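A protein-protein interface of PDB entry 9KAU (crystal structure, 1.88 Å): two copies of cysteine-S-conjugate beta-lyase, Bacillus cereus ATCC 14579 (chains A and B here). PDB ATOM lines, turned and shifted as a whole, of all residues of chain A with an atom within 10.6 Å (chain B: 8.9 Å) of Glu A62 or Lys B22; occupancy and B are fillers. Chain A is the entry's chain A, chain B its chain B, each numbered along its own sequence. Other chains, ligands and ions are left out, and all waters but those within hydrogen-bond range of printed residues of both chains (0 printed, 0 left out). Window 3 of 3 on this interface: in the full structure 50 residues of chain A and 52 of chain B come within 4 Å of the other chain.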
ATOM      1  N   THR A  58     -10.618  10.946 -27.293  1.00  0.00           N
ATOM      2  CA  THR A  58     -10.811  11.921 -26.237  1.00  0.00           C
ATOM      3  C   THR A  58      -9.636  12.882 -26.221  1.00  0.00           C
ATOM      4  O   THR A  58      -8.515  12.532 -26.610  1.00  0.00           O
ATOM      5  CB  THR A  58     -10.965  11.281 -24.837  1.00  0.00           C
ATOM      6  OG1 THR A  58      -9.710  10.764 -24.387  1.00  0.00           O
ATOM      7  CG2 THR A  58     -12.005  10.173 -24.849  1.00  0.00           C
ATOM      8  N   LEU A  59      -9.931  14.159 -25.782  1.00  0.00           N
ATOM      9  CA  LEU A  59      -8.985  15.223 -25.515  1.00  0.00           C
ATOM     10  C   LEU A  59      -8.459  15.097 -24.092  1.00  0.00           C
ATOM     11  O   LEU A  59      -9.178  14.654 -23.189  1.00  0.00           O
ATOM     12  CB  LEU A  59      -9.667  16.577 -25.663  1.00  0.00           C
ATOM     13  CG  LEU A  59     -10.417  16.942 -26.949  1.00  0.00           C
ATOM     14  CD1 LEU A  59     -11.767  17.599 -26.645  1.00  0.00           C
ATOM     15  CD2 LEU A  59      -9.565  17.853 -27.849  1.00  0.00           C
ATOM     16  N   PRO A  60      -7.248  15.590 -23.861  1.00  0.00           N
ATOM     17  CA  PRO A  60      -6.805  15.824 -22.488  1.00  0.00           C
ATOM     18  C   PRO A  60      -7.804  16.706 -21.756  1.00  0.00           C
ATOM     19  O   PRO A  60      -8.436  17.587 -22.366  1.00  0.00           O
ATOM     20  CB  PRO A  60      -5.461  16.544 -22.666  1.00  0.00           C
ATOM     21  CG  PRO A  60      -4.987  16.136 -24.039  1.00  0.00           C
ATOM     22  CD  PRO A  60      -6.184  15.763 -24.865  1.00  0.00           C
ATOM     23  N   PRO A  61      -8.024  16.457 -20.463  1.00  0.00           N
ATOM     24  CA  PRO A  61      -9.015  17.253 -19.717  1.00  0.00           C
ATOM     25  C   PRO A  61      -8.685  18.748 -19.712  1.00  0.00           C
ATOM     26  O   PRO A  61      -7.548  19.158 -19.947  1.00  0.00           O
ATOM     27  CB  PRO A  61      -8.954  16.655 -18.304  1.00  0.00           C
ATOM     28  CG  PRO A  61      -8.410  15.269 -18.504  1.00  0.00           C
ATOM     29  CD  PRO A  61      -7.419  15.410 -19.620  1.00  0.00           C
ATOM     30  N   GLU A  62      -9.722  19.571 -19.520  1.00  0.00           N
ATOM     31  CA  GLU A  62      -9.544  21.021 -19.552  1.00  0.00           C
ATOM     32  C   GLU A  62      -8.620  21.523 -18.439  1.00  0.00           C
ATOM     33  O   GLU A  62      -7.794  22.415 -18.667  1.00  0.00           O
ATOM     34  CB  GLU A  62     -10.906  21.712 -19.445  1.00  0.00           C
ATOM     35  CG  GLU A  62     -11.879  21.388 -20.550  1.00  0.00           C
ATOM     36  CD  GLU A  62     -13.218  22.077 -20.348  1.00  0.00           C
ATOM     37  OE1 GLU A  62     -13.517  22.467 -19.197  1.00  0.00           O
ATOM     38  OE2 GLU A  62     -13.970  22.227 -21.337  1.00  0.00           O
ATOM     39  N   ASN A  63      -8.759  20.982 -17.227  1.00  0.00           N
ATOM     40  CA  ASN A  63      -8.064  21.490 -16.046  1.00  0.00           C
ATOM     41  C   ASN A  63      -6.700  20.852 -15.833  1.00  0.00           C
ATOM     42  O   ASN A  63      -5.925  21.348 -15.007  1.00  0.00           O
ATOM     43  CB  ASN A  63      -8.918  21.266 -14.797  1.00  0.00           C
ATOM     44  CG  ASN A  63      -9.227  19.803 -14.574  1.00  0.00           C
ATOM     45  OD1 ASN A  63      -9.035  18.983 -15.469  1.00  0.00           O
ATOM     46  ND2 ASN A  63      -9.705  19.465 -13.386  1.00  0.00           N
ATOM     47  N   ILE A  64      -6.389  19.777 -16.563  1.00  0.00           N
ATOM     48  CA  ILE A  64      -5.249  18.917 -16.244  1.00  0.00           C
ATOM     49  C   ILE A  64      -3.942  19.709 -16.235  1.00  0.00           C
ATOM     50  O   ILE A  64      -2.971  19.313 -15.578  1.00  0.00           O
ATOM     51  CB  ILE A  64      -5.210  17.725 -17.231  1.00  0.00           C
ATOM     52  CG1 ILE A  64      -4.248  16.620 -16.769  1.00  0.00           C
ATOM     53  CG2 ILE A  64      -4.807  18.205 -18.621  1.00  0.00           C
ATOM     54  CD1 ILE A  64      -4.663  15.898 -15.525  1.00  0.00           C
ATOM     55  N   GLY A  65      -3.884  20.819 -16.973  1.00  0.00           N
ATOM     56  CA  GLY A  65      -2.694  21.656 -16.947  1.00  0.00           C
ATOM     57  C   GLY A  65      -2.532  22.410 -15.636  1.00  0.00           C
ATOM     58  O   GLY A  65      -1.410  22.659 -15.189  1.00  0.00           O
ATOM     59  N   ASP A  66      -3.643  22.865 -15.053  1.00  0.00           N
ATOM     60  CA  ASP A  66      -3.564  23.526 -13.757  1.00  0.00           C
ATOM     61  C   ASP A  66      -3.164  22.545 -12.679  1.00  0.00           C
ATOM     62  O   ASP A  66      -2.297  22.839 -11.843  1.00  0.00           O
ATOM     63  CB  ASP A  66      -4.899  24.144 -13.380  1.00  0.00           C
ATOM     64  CG  ASP A  66      -5.215  25.336 -14.184  1.00  0.00           C
ATOM     65  OD1 ASP A  66      -4.269  25.988 -14.658  1.00  0.00           O
ATOM     66  OD2 ASP A  66      -6.406  25.649 -14.303  1.00  0.00           O
ATOM     67  N   ILE A  67      -3.801  21.375 -12.686  1.00  0.00           N
ATOM     68  CA  ILE A  67      -3.506  20.349 -11.699  1.00  0.00           C
ATOM     69  C   ILE A  67      -2.037  19.960 -11.780  1.00  0.00           C
ATOM     70  O   ILE A  67      -1.357  19.825 -10.755  1.00  0.00           O
ATOM     71  CB  ILE A  67      -4.444  19.155 -11.917  1.00  0.00           C
ATOM     72  CG1 ILE A  67      -5.870  19.556 -11.542  1.00  0.00           C
ATOM     73  CG2 ILE A  67      -3.996  17.978 -11.106  1.00  0.00           C
ATOM     74  CD1 ILE A  67      -6.926  18.603 -12.031  1.00  0.00           C
ATOM     75  N   ILE A  68      -1.509  19.835 -12.999  1.00  0.00           N
ATOM     76  CA  ILE A  68      -0.107  19.465 -13.161  1.00  0.00           C
ATOM     77  C   ILE A  68       0.787  20.584 -12.666  1.00  0.00           C
ATOM     78  O   ILE A  68       1.765  20.348 -11.951  1.00  0.00           O
ATOM     79  CB  ILE A  68       0.174  19.103 -14.633  1.00  0.00           C
ATOM     80  CG1 ILE A  68      -0.429  17.742 -14.947  1.00  0.00           C
ATOM     81  CG2 ILE A  68       1.652  19.101 -14.946  1.00  0.00           C
ATOM     82  CD1 ILE A  68      -0.106  17.238 -16.329  1.00  0.00           C
ATOM     83  N   CYS A  69       0.421  21.822 -12.981  1.00  0.00           N
ATOM     84  CA  CYS A  69       1.157  22.988 -12.511  1.00  0.00           C
ATOM     85  C   CYS A  69       1.054  23.139 -11.011  1.00  0.00           C
ATOM     86  O   CYS A  69       2.000  23.584 -10.357  1.00  0.00           O
ATOM     87  CB  CYS A  69       0.556  24.231 -13.146  1.00  0.00           C
ATOM     88  SG  CYS A  69       1.349  24.933 -14.557  1.00  0.00           S
ATOM     89  N   ASN A  70      -0.113  22.813 -10.459  1.00  0.00           N
ATOM     90  CA  ASN A  70      -0.312  22.864  -9.016  1.00  0.00           C
ATOM     91  C   ASN A  70       0.496  21.769  -8.315  1.00  0.00           C
ATOM     92  O   ASN A  70       1.221  22.043  -7.349  1.00  0.00           O
ATOM     93  CB  ASN A  70      -1.812  22.763  -8.706  1.00  0.00           C
ATOM     94  CG  ASN A  70      -2.620  24.004  -9.182  1.00  0.00           C
ATOM     95  OD1 ASN A  70      -2.056  25.026  -9.605  1.00  0.00           O
ATOM     96  ND2 ASN A  70      -3.946  23.907  -9.101  1.00  0.00           N
ATOM     97  N   LYS A  82       1.832  26.016 -18.388  1.00  0.00           N
ATOM     98  CA  LYS A  82       1.018  25.012 -19.067  1.00  0.00           C
ATOM     99  C   LYS A  82       1.601  24.620 -20.414  1.00  0.00           C
ATOM    100  O   LYS A  82       1.318  23.525 -20.914  1.00  0.00           O
ATOM    101  CB  LYS A  82      -0.414  25.518 -19.258  1.00  0.00           C
ATOM    102  CG  LYS A  82      -1.344  25.186 -18.108  1.00  0.00           C
ATOM    103  CD  LYS A  82      -2.796  25.118 -18.536  1.00  0.00           C
ATOM    104  CE  LYS A  82      -3.656  26.099 -17.753  1.00  0.00           C
ATOM    105  NZ  LYS A  82      -5.119  25.899 -17.984  1.00  0.00           N
ATOM    106  N   ILE A  85       4.035  21.212 -20.576  1.00  0.00           N
ATOM    107  CA  ILE A  85       3.596  19.841 -20.350  1.00  0.00           C
ATOM    108  C   ILE A  85       3.444  19.139 -21.687  1.00  0.00           C
ATOM    109  O   ILE A  85       2.756  19.633 -22.588  1.00  0.00           O
ATOM    110  CB  ILE A  85       2.277  19.800 -19.584  1.00  0.00           C
ATOM    111  CG1 ILE A  85       2.346  20.733 -18.382  1.00  0.00           C
ATOM    112  CG2 ILE A  85       1.951  18.379 -19.212  1.00  0.00           C
ATOM    113  CD1 ILE A  85       0.995  21.101 -17.859  1.00  0.00           C
ATOM    114  N   PHE A  87       2.644  15.045 -23.025  1.00  0.00           N
ATOM    115  CA  PHE A  87       2.161  13.752 -22.563  1.00  0.00           C
ATOM    116  C   PHE A  87       2.944  12.629 -23.235  1.00  0.00           C
ATOM    117  O   PHE A  87       3.471  12.791 -24.335  1.00  0.00           O
ATOM    118  CB  PHE A  87       0.664  13.605 -22.824  1.00  0.00           C
ATOM    119  CG  PHE A  87      -0.179  14.462 -21.927  1.00  0.00           C
ATOM    120  CD1 PHE A  87      -0.544  14.020 -20.673  1.00  0.00           C
ATOM    121  CD2 PHE A  87      -0.569  15.730 -22.311  1.00  0.00           C
ATOM    122  CE1 PHE A  87      -1.300  14.819 -19.842  1.00  0.00           C
ATOM    123  CE2 PHE A  87      -1.319  16.523 -21.470  1.00  0.00           C
ATOM    124  CZ  PHE A  87      -1.679  16.070 -20.249  1.00  0.00           C
ATOM    125  N   TYR A 270      -5.673   9.449 -18.479  1.00  0.00           N
ATOM    126  CA  TYR A 270      -6.022  10.803 -18.087  1.00  0.00           C
ATOM    127  C   TYR A 270      -6.867  10.771 -16.822  1.00  0.00           C
ATOM    128  O   TYR A 270      -6.604  11.515 -15.871  1.00  0.00           O
ATOM    129  CB  TYR A 270      -6.800  11.528 -19.201  1.00  0.00           C
ATOM    130  CG  TYR A 270      -6.022  11.893 -20.453  1.00  0.00           C
ATOM    131  CD1 TYR A 270      -4.783  12.490 -20.387  1.00  0.00           C
ATOM    132  CD2 TYR A 270      -6.538  11.625 -21.697  1.00  0.00           C
ATOM    133  CE1 TYR A 270      -4.078  12.801 -21.535  1.00  0.00           C
ATOM    134  CE2 TYR A 270      -5.849  11.924 -22.834  1.00  0.00           C
ATOM    135  CZ  TYR A 270      -4.626  12.519 -22.762  1.00  0.00           C
ATOM    136  OH  TYR A 270      -3.969  12.815 -23.938  1.00  0.00           O
ATOM    137  N   THR A 271      -7.846   9.860 -16.771  1.00  0.00           N
ATOM    138  CA  THR A 271      -8.831   9.850 -15.695  1.00  0.00           C
ATOM    139  C   THR A 271      -8.192   9.531 -14.354  1.00  0.00           C
ATOM    140  O   THR A 271      -8.614  10.058 -13.318  1.00  0.00           O
ATOM    141  CB  THR A 271      -9.930   8.849 -16.026  1.00  0.00           C
ATOM    142  OG1 THR A 271     -10.351   9.038 -17.384  1.00  0.00           O
ATOM    143  CG2 THR A 271     -11.121   9.012 -15.097  1.00  0.00           C
ATOM    144  N   GLN A 274      -5.573  12.532 -13.376  1.00  0.00           N
ATOM    145  CA  GLN A 274      -6.246  13.744 -12.915  1.00  0.00           C
ATOM    146  C   GLN A 274      -6.624  13.644 -11.445  1.00  0.00           C
ATOM    147  O   GLN A 274      -6.521  14.625 -10.694  1.00  0.00           O
ATOM    148  CB  GLN A 274      -7.491  14.004 -13.762  1.00  0.00           C
ATOM    149  CG  GLN A 274      -8.251  15.257 -13.383  1.00  0.00           C
ATOM    150  CD  GLN A 274      -9.446  15.489 -14.280  1.00  0.00           C
ATOM    151  OE1 GLN A 274     -10.211  14.567 -14.563  1.00  0.00           O
ATOM    152  NE2 GLN A 274      -9.603  16.718 -14.751  1.00  0.00           N
ATOM    153  N   ARG B  11     -21.531  15.689 -24.994  1.00  0.00           N
ATOM    154  CA  ARG B  11     -20.908  16.924 -24.542  1.00  0.00           C
ATOM    155  C   ARG B  11     -20.521  16.778 -23.076  1.00  0.00           C
ATOM    156  O   ARG B  11     -21.229  16.136 -22.297  1.00  0.00           O
ATOM    157  CB  ARG B  11     -21.850  18.114 -24.733  1.00  0.00           C
ATOM    158  CG  ARG B  11     -22.146  18.437 -26.185  1.00  0.00           C
ATOM    159  CD  ARG B  11     -22.338  19.929 -26.405  1.00  0.00           C
ATOM    160  NE  ARG B  11     -22.776  20.223 -27.766  1.00  0.00           N
ATOM    161  CZ  ARG B  11     -21.948  20.519 -28.762  1.00  0.00           C
ATOM    162  NH1 ARG B  11     -20.638  20.554 -28.550  1.00  0.00           N
ATOM    163  NH2 ARG B  11     -22.427  20.779 -29.970  1.00  0.00           N
ATOM    164  N   GLY B  12     -19.366  17.337 -22.716  1.00  0.00           N
ATOM    165  CA  GLY B  12     -18.868  17.232 -21.359  1.00  0.00           C
ATOM    166  C   GLY B  12     -18.243  15.899 -21.031  1.00  0.00           C
ATOM    167  O   GLY B  12     -18.181  15.526 -19.855  1.00  0.00           O
ATOM    168  N   THR B  13     -17.786  15.157 -22.042  1.00  0.00           N
ATOM    169  CA  THR B  13     -17.170  13.849 -21.857  1.00  0.00           C
ATOM    170  C   THR B  13     -15.714  13.832 -22.307  1.00  0.00           C
ATOM    171  O   THR B  13     -15.105  12.754 -22.368  1.00  0.00           O
ATOM    172  CB  THR B  13     -17.958  12.766 -22.612  1.00  0.00           C
ATOM    173  OG1 THR B  13     -17.783  12.926 -24.026  1.00  0.00           O
ATOM    174  CG2 THR B  13     -19.447  12.850 -22.293  1.00  0.00           C
ATOM    175  N   HIS B  14     -15.154  15.005 -22.625  1.00  0.00           N
ATOM    176  CA  HIS B  14     -13.825  15.192 -23.205  1.00  0.00           C
ATOM    177  C   HIS B  14     -13.665  14.436 -24.526  1.00  0.00           C
ATOM    178  O   HIS B  14     -12.557  14.345 -25.074  1.00  0.00           O
ATOM    179  CB  HIS B  14     -12.730  14.826 -22.192  1.00  0.00           C
ATOM    180  CG  HIS B  14     -12.850  15.580 -20.898  1.00  0.00           C
ATOM    181  ND1 HIS B  14     -12.845  16.957 -20.835  1.00  0.00           N
ATOM    182  CD2 HIS B  14     -13.027  15.149 -19.626  1.00  0.00           C
ATOM    183  CE1 HIS B  14     -12.995  17.340 -19.581  1.00  0.00           C
ATOM    184  NE2 HIS B  14     -13.108  16.263 -18.829  1.00  0.00           N
ATOM    185  N   ILE B  16     -13.361  14.245 -28.319  1.00  0.00           N
ATOM    186  CA  ILE B  16     -12.920  15.202 -29.332  1.00  0.00           C
ATOM    187  C   ILE B  16     -14.084  15.628 -30.227  1.00  0.00           C
ATOM    188  O   ILE B  16     -14.152  16.778 -30.668  1.00  0.00           O
ATOM    189  CB  ILE B  16     -11.742  14.630 -30.147  1.00  0.00           C
ATOM    190  CG1 ILE B  16     -10.523  14.387 -29.242  1.00  0.00           C
ATOM    191  CG2 ILE B  16     -11.391  15.552 -31.321  1.00  0.00           C
ATOM    192  CD1 ILE B  16      -9.162  14.460 -29.938  1.00  0.00           C
ATOM    193  N   LYS B  17     -15.014  14.715 -30.513  1.00  0.00           N
ATOM    194  CA  LYS B  17     -16.105  15.033 -31.433  1.00  0.00           C
ATOM    195  C   LYS B  17     -17.049  16.066 -30.850  1.00  0.00           C
ATOM    196  O   LYS B  17     -17.444  17.019 -31.532  1.00  0.00           O
ATOM    197  CB  LYS B  17     -16.885  13.773 -31.806  1.00  0.00           C
ATOM    198  CG  LYS B  17     -17.559  13.898 -33.157  1.00  0.00           C
ATOM    199  CD  LYS B  17     -18.750  12.971 -33.315  1.00  0.00           C
ATOM    200  CE  LYS B  17     -19.213  12.949 -34.766  1.00  0.00           C
ATOM    201  NZ  LYS B  17     -19.595  11.596 -35.262  1.00  0.00           N
ATOM    202  N   TRP B  18     -17.437  15.882 -29.595  1.00  0.00           N
ATOM    203  CA  TRP B  18     -18.525  16.641 -28.987  1.00  0.00           C
ATOM    204  C   TRP B  18     -18.054  17.732 -28.042  1.00  0.00           C
ATOM    205  O   TRP B  18     -18.862  18.579 -27.647  1.00  0.00           O
ATOM    206  CB  TRP B  18     -19.484  15.687 -28.260  1.00  0.00           C
ATOM    207  CG  TRP B  18     -20.308  14.981 -29.263  1.00  0.00           C
ATOM    208  CD1 TRP B  18     -20.121  13.712 -29.735  1.00  0.00           C
ATOM    209  CD2 TRP B  18     -21.411  15.528 -30.000  1.00  0.00           C
ATOM    210  NE1 TRP B  18     -21.062  13.426 -30.696  1.00  0.00           N
ATOM    211  CE2 TRP B  18     -21.862  14.525 -30.880  1.00  0.00           C
ATOM    212  CE3 TRP B  18     -22.068  16.761 -29.988  1.00  0.00           C
ATOM    213  CZ2 TRP B  18     -22.943  14.716 -31.736  1.00  0.00           C
ATOM    214  CZ3 TRP B  18     -23.145  16.947 -30.849  1.00  0.00           C
ATOM    215  CH2 TRP B  18     -23.569  15.931 -31.706  1.00  0.00           C
ATOM    216  N   ASP B  19     -16.788  17.733 -27.653  1.00  0.00           N
ATOM    217  CA  ASP B  19     -16.335  18.703 -26.674  1.00  0.00           C
ATOM    218  C   ASP B  19     -15.301  19.681 -27.204  1.00  0.00           C
ATOM    219  O   ASP B  19     -15.067  20.706 -26.557  1.00  0.00           O
ATOM    220  CB  ASP B  19     -15.781  17.958 -25.453  1.00  0.00           C
ATOM    221  CG  ASP B  19     -16.877  17.270 -24.662  1.00  0.00           C
ATOM    222  OD1 ASP B  19     -17.928  17.894 -24.437  1.00  0.00           O
ATOM    223  OD2 ASP B  19     -16.713  16.090 -24.307  1.00  0.00           O
ATOM    224  N   THR B  20     -14.773  19.478 -28.410  1.00  0.00           N
ATOM    225  CA  THR B  20     -13.753  20.399 -28.886  1.00  0.00           C
ATOM    226  C   THR B  20     -14.341  21.768 -29.196  1.00  0.00           C
ATOM    227  O   THR B  20     -13.680  22.791 -28.979  1.00  0.00           O
ATOM    228  CB  THR B  20     -13.062  19.821 -30.107  1.00  0.00           C
ATOM    229  OG1 THR B  20     -12.648  18.482 -29.813  1.00  0.00           O
ATOM    230  CG2 THR B  20     -11.840  20.647 -30.464  1.00  0.00           C
ATOM    231  N   TYR B  21     -15.579  21.807 -29.682  1.00  0.00           N
ATOM    232  CA  TYR B  21     -16.322  23.044 -29.861  1.00  0.00           C
ATOM    233  C   TYR B  21     -17.305  23.206 -28.712  1.00  0.00           C
ATOM    234  O   TYR B  21     -17.992  22.251 -28.329  1.00  0.00           O
ATOM    235  CB  TYR B  21     -17.103  23.031 -31.170  1.00  0.00           C
ATOM    236  CG  TYR B  21     -16.291  23.028 -32.442  1.00  0.00           C
ATOM    237  CD1 TYR B  21     -15.678  21.871 -32.906  1.00  0.00           C
ATOM    238  CD2 TYR B  21     -16.184  24.171 -33.209  1.00  0.00           C
ATOM    239  CE1 TYR B  21     -14.960  21.869 -34.088  1.00  0.00           C
ATOM    240  CE2 TYR B  21     -15.470  24.172 -34.382  1.00  0.00           C
ATOM    241  CZ  TYR B  21     -14.861  23.024 -34.822  1.00  0.00           C
ATOM    242  OH  TYR B  21     -14.157  23.057 -36.007  1.00  0.00           O
ATOM    243  N   LYS B  22     -17.416  24.424 -28.198  1.00  0.00           N
ATOM    244  CA  LYS B  22     -18.279  24.653 -27.049  1.00  0.00           C
ATOM    245  C   LYS B  22     -19.616  25.295 -27.403  1.00  0.00           C
ATOM    246  O   LYS B  22     -20.530  25.269 -26.571  1.00  0.00           O
ATOM    247  CB  LYS B  22     -17.554  25.515 -26.000  1.00  0.00           C
ATOM    248  CG  LYS B  22     -16.315  24.861 -25.417  1.00  0.00           C
ATOM    249  CD  LYS B  22     -15.896  25.531 -24.133  1.00  0.00           C
ATOM    250  CE  LYS B  22     -15.326  24.524 -23.144  1.00  0.00           C
ATOM    251  NZ  LYS B  22     -15.097  25.122 -21.794  1.00  0.00           N
ATOM    252  N   ASN B  23     -19.790  25.806 -28.617  1.00  0.00           N
ATOM    253  CA  ASN B  23     -21.090  26.352 -28.993  1.00  0.00           C
ATOM    254  C   ASN B  23     -22.083  25.201 -29.120  1.00  0.00           C
ATOM    255  O   ASN B  23     -21.978  24.370 -30.027  1.00  0.00           O
ATOM    256  CB  ASN B  23     -20.993  27.147 -30.292  1.00  0.00           C
ATOM    257  CG  ASN B  23     -22.362  27.566 -30.835  1.00  0.00           C
ATOM    258  OD1 ASN B  23     -23.259  27.954 -30.084  1.00  0.00           O
ATOM    259  ND2 ASN B  23     -22.519  27.482 -32.149  1.00  0.00           N
ATOM    260  N   GLU B  24     -23.037  25.137 -28.194  1.00  0.00           N
ATOM    261  CA  GLU B  24     -23.952  24.005 -28.122  1.00  0.00           C
ATOM    262  C   GLU B  24     -24.914  23.954 -29.292  1.00  0.00           C
ATOM    263  O   GLU B  24     -25.733  23.030 -29.357  1.00  0.00           O
ATOM    264  CB  GLU B  24     -24.728  24.035 -26.806  1.00  0.00           C
ATOM    265  CG  GLU B  24     -23.836  24.234 -25.593  1.00  0.00           C
ATOM    266  CD  GLU B  24     -24.560  23.993 -24.289  1.00  0.00           C
ATOM    267  OE1 GLU B  24     -25.803  23.880 -24.298  1.00  0.00           O
ATOM    268  OE2 GLU B  24     -23.883  23.943 -23.248  1.00  0.00           O
ATOM    269  N   GLU B  25     -24.880  24.944 -30.180  1.00  0.00           N
ATOM    270  CA  GLU B  25     -25.699  24.905 -31.380  1.00  0.00           C
ATOM    271  C   GLU B  25     -25.113  24.014 -32.468  1.00  0.00           C
ATOM    272  O   GLU B  25     -25.822  23.674 -33.419  1.00  0.00           O
ATOM    273  CB  GLU B  25     -25.880  26.323 -31.922  1.00  0.00           C
ATOM    274  CG  GLU B  25     -27.242  26.914 -31.654  1.00  0.00           C
ATOM    275  CD  GLU B  25     -27.361  28.311 -32.208  1.00  0.00           C
ATOM    276  OE1 GLU B  25     -28.493  28.831 -32.294  1.00  0.00           O
ATOM    277  OE2 GLU B  25     -26.308  28.890 -32.553  1.00  0.00           O
ATOM    278  N   LEU B  26     -23.857  23.602 -32.340  1.00  0.00           N
ATOM    279  CA  LEU B  26     -23.193  22.864 -33.403  1.00  0.00           C
ATOM    280  C   LEU B  26     -23.589  21.395 -33.352  1.00  0.00           C
ATOM    281  O   LEU B  26     -23.854  20.844 -32.281  1.00  0.00           O
ATOM    282  CB  LEU B  26     -21.672  23.012 -33.305  1.00  0.00           C
ATOM    283  CG  LEU B  26     -21.166  24.429 -33.601  1.00  0.00           C
ATOM    284  CD1 LEU B  26     -19.687  24.576 -33.305  1.00  0.00           C
ATOM    285  CD2 LEU B  26     -21.469  24.823 -35.039  1.00  0.00           C
ATOM    286  N   HIS B  28     -22.041  17.790 -34.635  1.00  0.00           N
ATOM    287  CA  HIS B  28     -20.718  17.278 -34.965  1.00  0.00           C
ATOM    288  C   HIS B  28     -20.833  15.928 -35.658  1.00  0.00           C
ATOM    289  O   HIS B  28     -21.509  15.019 -35.157  1.00  0.00           O
ATOM    290  CB  HIS B  28     -19.852  17.158 -33.714  1.00  0.00           C
ATOM    291  CG  HIS B  28     -19.551  18.475 -33.078  1.00  0.00           C
ATOM    292  ND1 HIS B  28     -20.305  18.988 -32.044  1.00  0.00           N
ATOM    293  CD2 HIS B  28     -18.591  19.392 -33.337  1.00  0.00           C
ATOM    294  CE1 HIS B  28     -19.816  20.161 -31.688  1.00  0.00           C
ATOM    295  NE2 HIS B  28     -18.776  20.429 -32.457  1.00  0.00           N
ATOM    296  N   ILE B 345     -20.658  20.477 -38.141  1.00  0.00           N
ATOM    297  CA  ILE B 345     -19.218  20.334 -38.331  1.00  0.00           C
ATOM    298  C   ILE B 345     -18.937  19.044 -39.077  1.00  0.00           C
ATOM    299  O   ILE B 345     -19.223  17.945 -38.577  1.00  0.00           O
ATOM    300  CB  ILE B 345     -18.454  20.337 -37.005  1.00  0.00           C
ATOM    301  CG1 ILE B 345     -18.769  21.616 -36.214  1.00  0.00           C
ATOM    302  CG2 ILE B 345     -16.972  20.117 -37.286  1.00  0.00           C
ATOM    303  CD1 ILE B 345     -18.575  22.932 -36.967  1.00  0.00           C
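N of Leu A59 sits at hydrogen-bond distance from O of His B14, at 2.7 Å.
NZ of Lys B22 is in salt-bridge range of OE2 of Glu A62, 3.1 Å away.
The backbone carbonyl oxygen of Ile B16 is in hydrogen-bond range of the side-chain hydroxyl of Thr B20 (2.4 Å).
The backbone NH (N) of His B14 is in hydrogen-bond range of the side-chain carboxylate (OD2) of Asp B19.
Among the printed residues, pairs that only touch across the chains: Thr A58 with His B14 (3.2 Å), Leu A59 with Thr B20 (3.4 Å), Leu A59 with Ile B16 (3.4 Å), Thr A58 with Ile B16 (3.5 Å), Glu A62 with His B14 (3.96 Å) and Pro A61 with His B14 (3.98 Å).
Glu A62 touches two residues of chain B.
Printed residues of chain A within 4 Å of Lys B22: Glu A62.
No residue of chain A comes within 4 Å of Glu B24.
Printed residues of chain A within 4 Å of Thr B20: Leu A59 (3.4 Å).
Printed residues of chain A within 4 Å of His B14: Thr A58 (3.2 Å), Leu A59 (2.7 Å), Pro A61 (3.98 Å) and Glu A62 (3.96 Å).
Lys A82 touches none of the printed residues of chain B.
Trp B18 touches none of the printed residues of chain A.
The nearest residue of chain B that does not touch Glu A62 is Asp B19 (5.5 Å).
The nearest residue of chain A that does not touch Lys B22 is Leu A59 (8.5 Å).
Of the 17 printed residues of chain B, 4 touch a printed residue of chain A.
Hydrophobic or aromatic side chains of chain B within 4 Å of the printed part of chain A: His B14 and Ile B16.
Of the 19 printed residues of chain A, 4 touch a printed residue of chain B.
No position is printed for both chains.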
